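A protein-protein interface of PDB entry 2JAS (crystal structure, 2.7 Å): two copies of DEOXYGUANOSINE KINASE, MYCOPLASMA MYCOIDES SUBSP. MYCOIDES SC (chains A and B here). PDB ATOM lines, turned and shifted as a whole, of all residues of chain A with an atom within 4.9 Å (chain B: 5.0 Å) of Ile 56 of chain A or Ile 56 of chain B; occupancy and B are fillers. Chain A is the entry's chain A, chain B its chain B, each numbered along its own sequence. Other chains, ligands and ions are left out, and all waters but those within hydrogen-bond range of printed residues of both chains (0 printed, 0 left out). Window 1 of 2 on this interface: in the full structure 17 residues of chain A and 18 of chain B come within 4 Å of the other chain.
Among the printed residues, pairs that only touch across the chains: Phe 52 of chain A with Ile 56 of chain B (3.8 Å), Lys 53 of chain A with Phe 52 of chain B (3.7 Å), Ile 56 of chain A with Phe 52 of chain B (3.3 Å), Ile 56 of chain A with Ile 56 of chain B (3.8 Å), Ile 56 of chain A with Thr 104 of chain B (3.8 Å), Ile 56 of chain A with Phe 108 of chain B (3.7 Å), Tyr 57 of chain A with Thr 104 of chain B (3.8 Å), Thr 60 of chain A with Phe 108 of chain B (3.5 Å), Thr 104 of chain A with Ile 56 of chain B (3.8 Å), Thr 104 of chain A with Tyr 57 of chain B (3.8 Å), Phe 108 of chain A with Ile 56 of chain B (3.7 Å), Phe 108 of chain A with Thr 60 of chain B (3.2 Å) and Phe 108 of chain A with Phe 108 of chain B (3.1 Å).
O of Ile 56 of chain B sits at hydrogen-bond distance from OG1 of Thr 60 of chain B, at 2.8 Å. The side-chain hydroxyl of Thr 60 of chain A lies within hydrogen-bond range of the backbone carbonyl oxygen of Ile 56 of chain A (2.5 Å).
Printed residues of chain B that touch a printed residue of chain A: Phe 52, Ile 56, Tyr 57, Thr 60, Thr 104 and Phe 108. Hydrophobic or aromatic side chains of chain B that line the printed part of chain A: Phe 52, Ile 56, Tyr 57 and Phe 108. Among the printed residues, no Asp or Glu carboxylate lies within 4 Å of a Lys or Arg side-chain nitrogen of the other chain.
Lys 53 of chain A touches Phe 52 of chain B, but with the chains exchanged Phe 52 of chain A does not touch Lys 53 of chain B (4.5 Å). Ile 56 of chain A touches Thr 104 of chain B, and with the chains exchanged Thr 104 of chain A touches Ile 56 of chain B. Tyr 57 of chain A touches Thr 104 of chain B, and with the chains exchanged Thr 104 of chain A touches Tyr 57 of chain B. Phe 108 of chain B touches its own counterpart, Phe 108 of chain A. Of the 13 pairs that touch across the chains among the printed residues, 12 have their exchanged pair printed and touching as well.
Of the printed residues of chain B, Ile 56 of chain A touches Phe 52 (3.3 Å), Ile 56 (3.8 Å), Thr 104 (3.8 Å) and Phe 108 (3.7 Å). Ile 56 of chain B touches just these residues of chain A: Phe 52, Ile 56, Thr 104 and Phe 108. Printed residues of chain A within 4 Å of Thr 60 of chain B: Phe 108. Printed residues of chain A within 4 Å of Phe 52 of chain B: Lys 53 and Ile 56. Printed residues of chain A within 4 Å of Thr 104 of chain B: Ile 56 (3.8 Å) and Tyr 57 (3.8 Å). Leu 59 of chain B touches none of the printed residues of chain A. Gln 55 of chain B touches none of the printed residues of chain A. The nearest residue of chain A that does not touch Ile 56 of chain B is Tyr 105 of chain A (4.8 Å).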
ATOM      1  N   PHE A  52     -13.775 -25.700 -11.600  1.00  0.00           N
ATOM      2  CA  PHE A  52     -12.850 -24.573 -11.548  1.00  0.00           C
ATOM      3  C   PHE A  52     -12.430 -24.227 -10.128  1.00  0.00           C
ATOM      4  O   PHE A  52     -11.238 -24.056  -9.856  1.00  0.00           O
ATOM      5  CB  PHE A  52     -13.394 -23.357 -12.313  1.00  0.00           C
ATOM      6  CG  PHE A  52     -13.015 -23.363 -13.763  1.00  0.00           C
ATOM      7  CD1 PHE A  52     -13.843 -23.960 -14.710  1.00  0.00           C
ATOM      8  CD2 PHE A  52     -11.796 -22.820 -14.179  1.00  0.00           C
ATOM      9  CE1 PHE A  52     -13.475 -23.999 -16.055  1.00  0.00           C
ATOM     10  CE2 PHE A  52     -11.417 -22.850 -15.521  1.00  0.00           C
ATOM     11  CZ  PHE A  52     -12.257 -23.440 -16.460  1.00  0.00           C
ATOM     12  N   LYS A  53     -13.414 -24.144  -9.231  1.00  0.00           N
ATOM     13  CA  LYS A  53     -13.160 -23.969  -7.802  1.00  0.00           C
ATOM     14  C   LYS A  53     -12.239 -25.077  -7.302  1.00  0.00           C
ATOM     15  O   LYS A  53     -11.266 -24.818  -6.594  1.00  0.00           O
ATOM     16  CB  LYS A  53     -14.468 -23.995  -7.012  1.00  0.00           C
ATOM     17  CG  LYS A  53     -15.303 -22.715  -7.079  1.00  0.00           C
ATOM     18  CD  LYS A  53     -16.673 -22.929  -6.428  1.00  0.00           C
ATOM     19  CE  LYS A  53     -17.311 -21.608  -6.045  1.00  0.00           C
ATOM     20  NZ  LYS A  53     -18.772 -21.703  -5.767  1.00  0.00           N
ATOM     21  N   MET A  54     -12.550 -26.310  -7.696  1.00  0.00           N
ATOM     22  CA  MET A  54     -11.785 -27.473  -7.279  1.00  0.00           C
ATOM     23  C   MET A  54     -10.349 -27.351  -7.749  1.00  0.00           C
ATOM     24  O   MET A  54      -9.422 -27.550  -6.963  1.00  0.00           O
ATOM     25  CB  MET A  54     -12.408 -28.766  -7.817  1.00  0.00           C
ATOM     26  CG  MET A  54     -11.683 -30.049  -7.383  1.00  0.00           C
ATOM     27  SD  MET A  54     -11.735 -30.361  -5.598  1.00  0.00           S
ATOM     28  CE  MET A  54     -10.863 -31.928  -5.506  1.00  0.00           C
ATOM     29  N   GLN A  55     -10.184 -27.024  -9.030  1.00  0.00           N
ATOM     30  CA  GLN A  55      -8.867 -26.922  -9.653  1.00  0.00           C
ATOM     31  C   GLN A  55      -7.992 -25.859  -8.987  1.00  0.00           C
ATOM     32  O   GLN A  55      -6.828 -26.126  -8.656  1.00  0.00           O
ATOM     33  CB  GLN A  55      -8.994 -26.668 -11.162  1.00  0.00           C
ATOM     34  CG  GLN A  55      -9.218 -27.931 -11.978  1.00  0.00           C
ATOM     35  CD  GLN A  55      -8.135 -28.988 -11.740  1.00  0.00           C
ATOM     36  OE1 GLN A  55      -8.437 -30.132 -11.406  1.00  0.00           O
ATOM     37  NE2 GLN A  55      -6.871 -28.601 -11.898  1.00  0.00           N
ATOM     38  N   ILE A  56      -8.568 -24.674  -8.774  1.00  0.00           N
ATOM     39  CA  ILE A  56      -7.858 -23.569  -8.143  1.00  0.00           C
ATOM     40  C   ILE A  56      -7.340 -23.958  -6.760  1.00  0.00           C
ATOM     41  O   ILE A  56      -6.191 -23.672  -6.424  1.00  0.00           O
ATOM     42  CB  ILE A  56      -8.725 -22.305  -8.075  1.00  0.00           C
ATOM     43  CG1 ILE A  56      -8.938 -21.754  -9.489  1.00  0.00           C
ATOM     44  CG2 ILE A  56      -8.075 -21.245  -7.182  1.00  0.00           C
ATOM     45  CD1 ILE A  56      -9.913 -20.606  -9.564  1.00  0.00           C
ATOM     46  N   TYR A  57      -8.180 -24.631  -5.976  1.00  0.00           N
ATOM     47  CA  TYR A  57      -7.772 -25.137  -4.671  1.00  0.00           C
ATOM     48  C   TYR A  57      -6.608 -26.109  -4.788  1.00  0.00           C
ATOM     49  O   TYR A  57      -5.637 -26.025  -4.032  1.00  0.00           O
ATOM     50  CB  TYR A  57      -8.935 -25.820  -3.935  1.00  0.00           C
ATOM     51  CG  TYR A  57      -8.551 -26.259  -2.540  1.00  0.00           C
ATOM     52  CD1 TYR A  57      -8.601 -25.367  -1.475  1.00  0.00           C
ATOM     53  CD2 TYR A  57      -8.108 -27.554  -2.291  1.00  0.00           C
ATOM     54  CE1 TYR A  57      -8.232 -25.755  -0.191  1.00  0.00           C
ATOM     55  CE2 TYR A  57      -7.734 -27.958  -1.013  1.00  0.00           C
ATOM     56  CZ  TYR A  57      -7.801 -27.050   0.033  1.00  0.00           C
ATOM     57  OH  TYR A  57      -7.439 -27.432   1.305  1.00  0.00           O
ATOM     58  N   MET A  58      -6.713 -27.032  -5.735  1.00  0.00           N
ATOM     59  CA  MET A  58      -5.723 -28.094  -5.868  1.00  0.00           C
ATOM     60  C   MET A  58      -4.340 -27.577  -6.257  1.00  0.00           C
ATOM     61  O   MET A  58      -3.359 -27.963  -5.629  1.00  0.00           O
ATOM     62  CB  MET A  58      -6.214 -29.187  -6.817  1.00  0.00           C
ATOM     63  CG  MET A  58      -7.425 -29.961  -6.306  1.00  0.00           C
ATOM     64  SD  MET A  58      -7.016 -31.177  -5.031  1.00  0.00           S
ATOM     65  CE  MET A  58      -7.130 -30.212  -3.547  1.00  0.00           C
ATOM     66  N   LEU A  59      -4.264 -26.691  -7.254  1.00  0.00           N
ATOM     67  CA  LEU A  59      -2.980 -26.118  -7.679  1.00  0.00           C
ATOM     68  C   LEU A  59      -2.359 -25.299  -6.551  1.00  0.00           C
ATOM     69  O   LEU A  59      -1.137 -25.255  -6.393  1.00  0.00           O
ATOM     70  CB  LEU A  59      -3.129 -25.245  -8.932  1.00  0.00           C
ATOM     71  CG  LEU A  59      -3.878 -25.772 -10.166  1.00  0.00           C
ATOM     72  CD1 LEU A  59      -4.397 -24.611 -11.021  1.00  0.00           C
ATOM     73  CD2 LEU A  59      -3.051 -26.747 -11.003  1.00  0.00           C
ATOM     74  N   THR A  60      -3.216 -24.655  -5.767  1.00  0.00           N
ATOM     75  CA  THR A  60      -2.779 -23.901  -4.608  1.00  0.00           C
ATOM     76  C   THR A  60      -2.146 -24.852  -3.603  1.00  0.00           C
ATOM     77  O   THR A  60      -1.050 -24.598  -3.110  1.00  0.00           O
ATOM     78  CB  THR A  60      -3.945 -23.121  -3.977  1.00  0.00           C
ATOM     79  OG1 THR A  60      -4.589 -22.342  -4.992  1.00  0.00           O
ATOM     80  CG2 THR A  60      -3.454 -22.193  -2.870  1.00  0.00           C
ATOM     81  N   THR A 104      -8.779 -22.326 -21.698  1.00  0.00           N
ATOM     82  CA  THR A 104      -8.464 -21.335 -20.687  1.00  0.00           C
ATOM     83  C   THR A 104      -7.640 -21.984 -19.569  1.00  0.00           C
ATOM     84  O   THR A 104      -6.575 -21.483 -19.210  1.00  0.00           O
ATOM     85  CB  THR A 104      -9.742 -20.673 -20.151  1.00  0.00           C
ATOM     86  OG1 THR A 104     -10.478 -20.120 -21.250  1.00  0.00           O
ATOM     87  CG2 THR A 104      -9.410 -19.549 -19.188  1.00  0.00           C
ATOM     88  N   TYR A 105      -8.107 -23.118 -19.054  1.00  0.00           N
ATOM     89  CA  TYR A 105      -7.371 -23.835 -18.015  1.00  0.00           C
ATOM     90  C   TYR A 105      -5.915 -24.126 -18.402  1.00  0.00           C
ATOM     91  O   TYR A 105      -5.000 -23.771 -17.660  1.00  0.00           O
ATOM     92  CB  TYR A 105      -8.083 -25.129 -17.603  1.00  0.00           C
ATOM     93  CG  TYR A 105      -7.285 -25.970 -16.619  1.00  0.00           C
ATOM     94  CD1 TYR A 105      -7.299 -25.689 -15.245  1.00  0.00           C
ATOM     95  CD2 TYR A 105      -6.504 -27.037 -17.060  1.00  0.00           C
ATOM     96  CE1 TYR A 105      -6.561 -26.455 -14.341  1.00  0.00           C
ATOM     97  CE2 TYR A 105      -5.769 -27.813 -16.166  1.00  0.00           C
ATOM     98  CZ  TYR A 105      -5.801 -27.517 -14.812  1.00  0.00           C
ATOM     99  OH  TYR A 105      -5.065 -28.290 -13.940  1.00  0.00           O
ATOM    100  N   PHE A 108      -3.617 -21.140 -18.990  1.00  0.00           N
ATOM    101  CA  PHE A 108      -3.187 -20.655 -17.685  1.00  0.00           C
ATOM    102  C   PHE A 108      -2.101 -21.535 -17.073  1.00  0.00           C
ATOM    103  O   PHE A 108      -1.117 -21.030 -16.528  1.00  0.00           O
ATOM    104  CB  PHE A 108      -4.376 -20.560 -16.721  1.00  0.00           C
ATOM    105  CG  PHE A 108      -3.978 -20.224 -15.314  1.00  0.00           C
ATOM    106  CD1 PHE A 108      -3.782 -18.901 -14.934  1.00  0.00           C
ATOM    107  CD2 PHE A 108      -3.768 -21.235 -14.379  1.00  0.00           C
ATOM    108  CE1 PHE A 108      -3.399 -18.583 -13.642  1.00  0.00           C
ATOM    109  CE2 PHE A 108      -3.382 -20.928 -13.083  1.00  0.00           C
ATOM    110  CZ  PHE A 108      -3.194 -19.596 -12.717  1.00  0.00           C
ATOM    111  N   PHE B  52     -15.002 -17.087 -11.736  1.00  0.00           N
ATOM    112  CA  PHE B  52     -13.779 -17.902 -11.775  1.00  0.00           C
ATOM    113  C   PHE B  52     -13.185 -18.087 -13.178  1.00  0.00           C
ATOM    114  O   PHE B  52     -11.981 -17.897 -13.364  1.00  0.00           O
ATOM    115  CB  PHE B  52     -13.982 -19.256 -11.058  1.00  0.00           C
ATOM    116  CG  PHE B  52     -13.966 -19.139  -9.561  1.00  0.00           C
ATOM    117  CD1 PHE B  52     -15.157 -19.090  -8.838  1.00  0.00           C
ATOM    118  CD2 PHE B  52     -12.756 -19.021  -8.877  1.00  0.00           C
ATOM    119  CE1 PHE B  52     -15.142 -18.946  -7.455  1.00  0.00           C
ATOM    120  CE2 PHE B  52     -12.726 -18.878  -7.495  1.00  0.00           C
ATOM    121  CZ  PHE B  52     -13.919 -18.843  -6.782  1.00  0.00           C
ATOM    122  N   LYS B  53     -14.026 -18.450 -14.149  1.00  0.00           N
ATOM    123  CA  LYS B  53     -13.600 -18.539 -15.555  1.00  0.00           C
ATOM    124  C   LYS B  53     -12.963 -17.225 -16.024  1.00  0.00           C
ATOM    125  O   LYS B  53     -11.866 -17.224 -16.582  1.00  0.00           O
ATOM    126  CB  LYS B  53     -14.784 -18.869 -16.480  1.00  0.00           C
ATOM    127  CG  LYS B  53     -15.615 -20.080 -16.080  1.00  0.00           C
ATOM    128  CD  LYS B  53     -16.855 -20.210 -16.974  1.00  0.00           C
ATOM    129  CE  LYS B  53     -17.697 -21.433 -16.586  1.00  0.00           C
ATOM    130  NZ  LYS B  53     -18.892 -21.593 -17.463  1.00  0.00           N
ATOM    131  N   MET B  54     -13.671 -16.118 -15.801  1.00  0.00           N
ATOM    132  CA  MET B  54     -13.200 -14.788 -16.176  1.00  0.00           C
ATOM    133  C   MET B  54     -11.821 -14.547 -15.585  1.00  0.00           C
ATOM    134  O   MET B  54     -10.852 -14.282 -16.302  1.00  0.00           O
ATOM    135  CB  MET B  54     -14.175 -13.725 -15.658  1.00  0.00           C
ATOM    136  CG  MET B  54     -13.843 -12.295 -16.066  1.00  0.00           C
ATOM    137  SD  MET B  54     -14.375 -11.934 -17.748  1.00  0.00           S
ATOM    138  CE  MET B  54     -13.930 -10.211 -17.895  1.00  0.00           C
ATOM    139  N   GLN B  55     -11.755 -14.670 -14.265  1.00  0.00           N
ATOM    140  CA  GLN B  55     -10.557 -14.423 -13.482  1.00  0.00           C
ATOM    141  C   GLN B  55      -9.319 -15.201 -13.966  1.00  0.00           C
ATOM    142  O   GLN B  55      -8.243 -14.618 -14.118  1.00  0.00           O
ATOM    143  CB  GLN B  55     -10.854 -14.722 -12.014  1.00  0.00           C
ATOM    144  CG  GLN B  55      -9.913 -14.059 -11.051  1.00  0.00           C
ATOM    145  CD  GLN B  55     -10.198 -12.588 -10.827  1.00  0.00           C
ATOM    146  OE1 GLN B  55     -11.273 -12.066 -11.157  1.00  0.00           O
ATOM    147  NE2 GLN B  55      -9.226 -11.906 -10.249  1.00  0.00           N
ATOM    148  N   ILE B  56      -9.470 -16.498 -14.218  1.00  0.00           N
ATOM    149  CA  ILE B  56      -8.360 -17.306 -14.743  1.00  0.00           C
ATOM    150  C   ILE B  56      -7.886 -16.829 -16.132  1.00  0.00           C
ATOM    151  O   ILE B  56      -6.684 -16.773 -16.409  1.00  0.00           O
ATOM    152  CB  ILE B  56      -8.690 -18.822 -14.723  1.00  0.00           C
ATOM    153  CG1 ILE B  56      -8.459 -19.373 -13.310  1.00  0.00           C
ATOM    154  CG2 ILE B  56      -7.838 -19.592 -15.739  1.00  0.00           C
ATOM    155  CD1 ILE B  56      -8.756 -20.851 -13.165  1.00  0.00           C
ATOM    156  N   TYR B  57      -8.841 -16.465 -16.980  1.00  0.00           N
ATOM    157  CA  TYR B  57      -8.546 -15.913 -18.302  1.00  0.00           C
ATOM    158  C   TYR B  57      -7.734 -14.617 -18.192  1.00  0.00           C
ATOM    159  O   TYR B  57      -6.684 -14.480 -18.829  1.00  0.00           O
ATOM    160  CB  TYR B  57      -9.839 -15.684 -19.099  1.00  0.00           C
ATOM    161  CG  TYR B  57      -9.593 -15.249 -20.514  1.00  0.00           C
ATOM    162  CD1 TYR B  57      -9.283 -16.180 -21.514  1.00  0.00           C
ATOM    163  CD2 TYR B  57      -9.661 -13.902 -20.865  1.00  0.00           C
ATOM    164  CE1 TYR B  57      -9.050 -15.771 -22.830  1.00  0.00           C
ATOM    165  CE2 TYR B  57      -9.427 -13.483 -22.169  1.00  0.00           C
ATOM    166  CZ  TYR B  57      -9.127 -14.418 -23.143  1.00  0.00           C
ATOM    167  OH  TYR B  57      -8.898 -13.989 -24.423  1.00  0.00           O
ATOM    168  N   MET B  58      -8.219 -13.685 -17.373  1.00  0.00           N
ATOM    169  CA  MET B  58      -7.554 -12.403 -17.182  1.00  0.00           C
ATOM    170  C   MET B  58      -6.164 -12.549 -16.562  1.00  0.00           C
ATOM    171  O   MET B  58      -5.241 -11.829 -16.947  1.00  0.00           O
ATOM    172  CB  MET B  58      -8.424 -11.459 -16.357  1.00  0.00           C
ATOM    173  CG  MET B  58      -9.703 -11.043 -17.076  1.00  0.00           C
ATOM    174  SD  MET B  58      -9.357 -10.041 -18.543  1.00  0.00           S
ATOM    175  CE  MET B  58     -10.480 -10.766 -19.727  1.00  0.00           C
ATOM    176  N   LEU B  59      -6.011 -13.484 -15.619  1.00  0.00           N
ATOM    177  CA  LEU B  59      -4.708 -13.723 -14.984  1.00  0.00           C
ATOM    178  C   LEU B  59      -3.669 -14.273 -15.974  1.00  0.00           C
ATOM    179  O   LEU B  59      -2.481 -13.946 -15.883  1.00  0.00           O
ATOM    180  CB  LEU B  59      -4.835 -14.633 -13.759  1.00  0.00           C
ATOM    181  CG  LEU B  59      -5.670 -14.164 -12.553  1.00  0.00           C
ATOM    182  CD1 LEU B  59      -5.995 -15.339 -11.624  1.00  0.00           C
ATOM    183  CD2 LEU B  59      -5.019 -13.011 -11.775  1.00  0.00           C
ATOM    184  N   THR B  60      -4.127 -15.089 -16.924  1.00  0.00           N
ATOM    185  CA  THR B  60      -3.276 -15.578 -18.006  1.00  0.00           C
ATOM    186  C   THR B  60      -2.802 -14.416 -18.873  1.00  0.00           C
ATOM    187  O   THR B  60      -1.622 -14.345 -19.234  1.00  0.00           O
ATOM    188  CB  THR B  60      -4.005 -16.612 -18.898  1.00  0.00           C
ATOM    189  OG1 THR B  60      -4.599 -17.621 -18.079  1.00  0.00           O
ATOM    190  CG2 THR B  60      -3.037 -17.278 -19.864  1.00  0.00           C
ATOM    191  N   THR B 104      -9.572 -18.986  -0.895  1.00  0.00           N
ATOM    192  CA  THR B 104      -8.864 -19.855  -1.834  1.00  0.00           C
ATOM    193  C   THR B 104      -8.181 -18.996  -2.900  1.00  0.00           C
ATOM    194  O   THR B 104      -7.020 -19.219  -3.240  1.00  0.00           O
ATOM    195  CB  THR B 104      -9.820 -20.911  -2.461  1.00  0.00           C
ATOM    196  OG1 THR B 104     -10.282 -21.799  -1.430  1.00  0.00           O
ATOM    197  CG2 THR B 104      -9.115 -21.736  -3.534  1.00  0.00           C
ATOM    198  N   PHE B 108      -4.459 -18.422  -3.523  1.00  0.00           N
ATOM    199  CA  PHE B 108      -4.032 -18.754  -4.869  1.00  0.00           C
ATOM    200  C   PHE B 108      -3.182 -17.628  -5.463  1.00  0.00           C
ATOM    201  O   PHE B 108      -2.122 -17.878  -6.047  1.00  0.00           O
ATOM    202  CB  PHE B 108      -5.277 -19.016  -5.719  1.00  0.00           C
ATOM    203  CG  PHE B 108      -5.007 -19.157  -7.180  1.00  0.00           C
ATOM    204  CD1 PHE B 108      -4.190 -20.175  -7.660  1.00  0.00           C
ATOM    205  CD2 PHE B 108      -5.602 -18.285  -8.086  1.00  0.00           C
ATOM    206  CE1 PHE B 108      -3.951 -20.308  -9.012  1.00  0.00           C
ATOM    207  CE2 PHE B 108      -5.372 -18.416  -9.449  1.00  0.00           C
ATOM    208  CZ  PHE B 108      -4.544 -19.429  -9.906  1.00  0.00           C
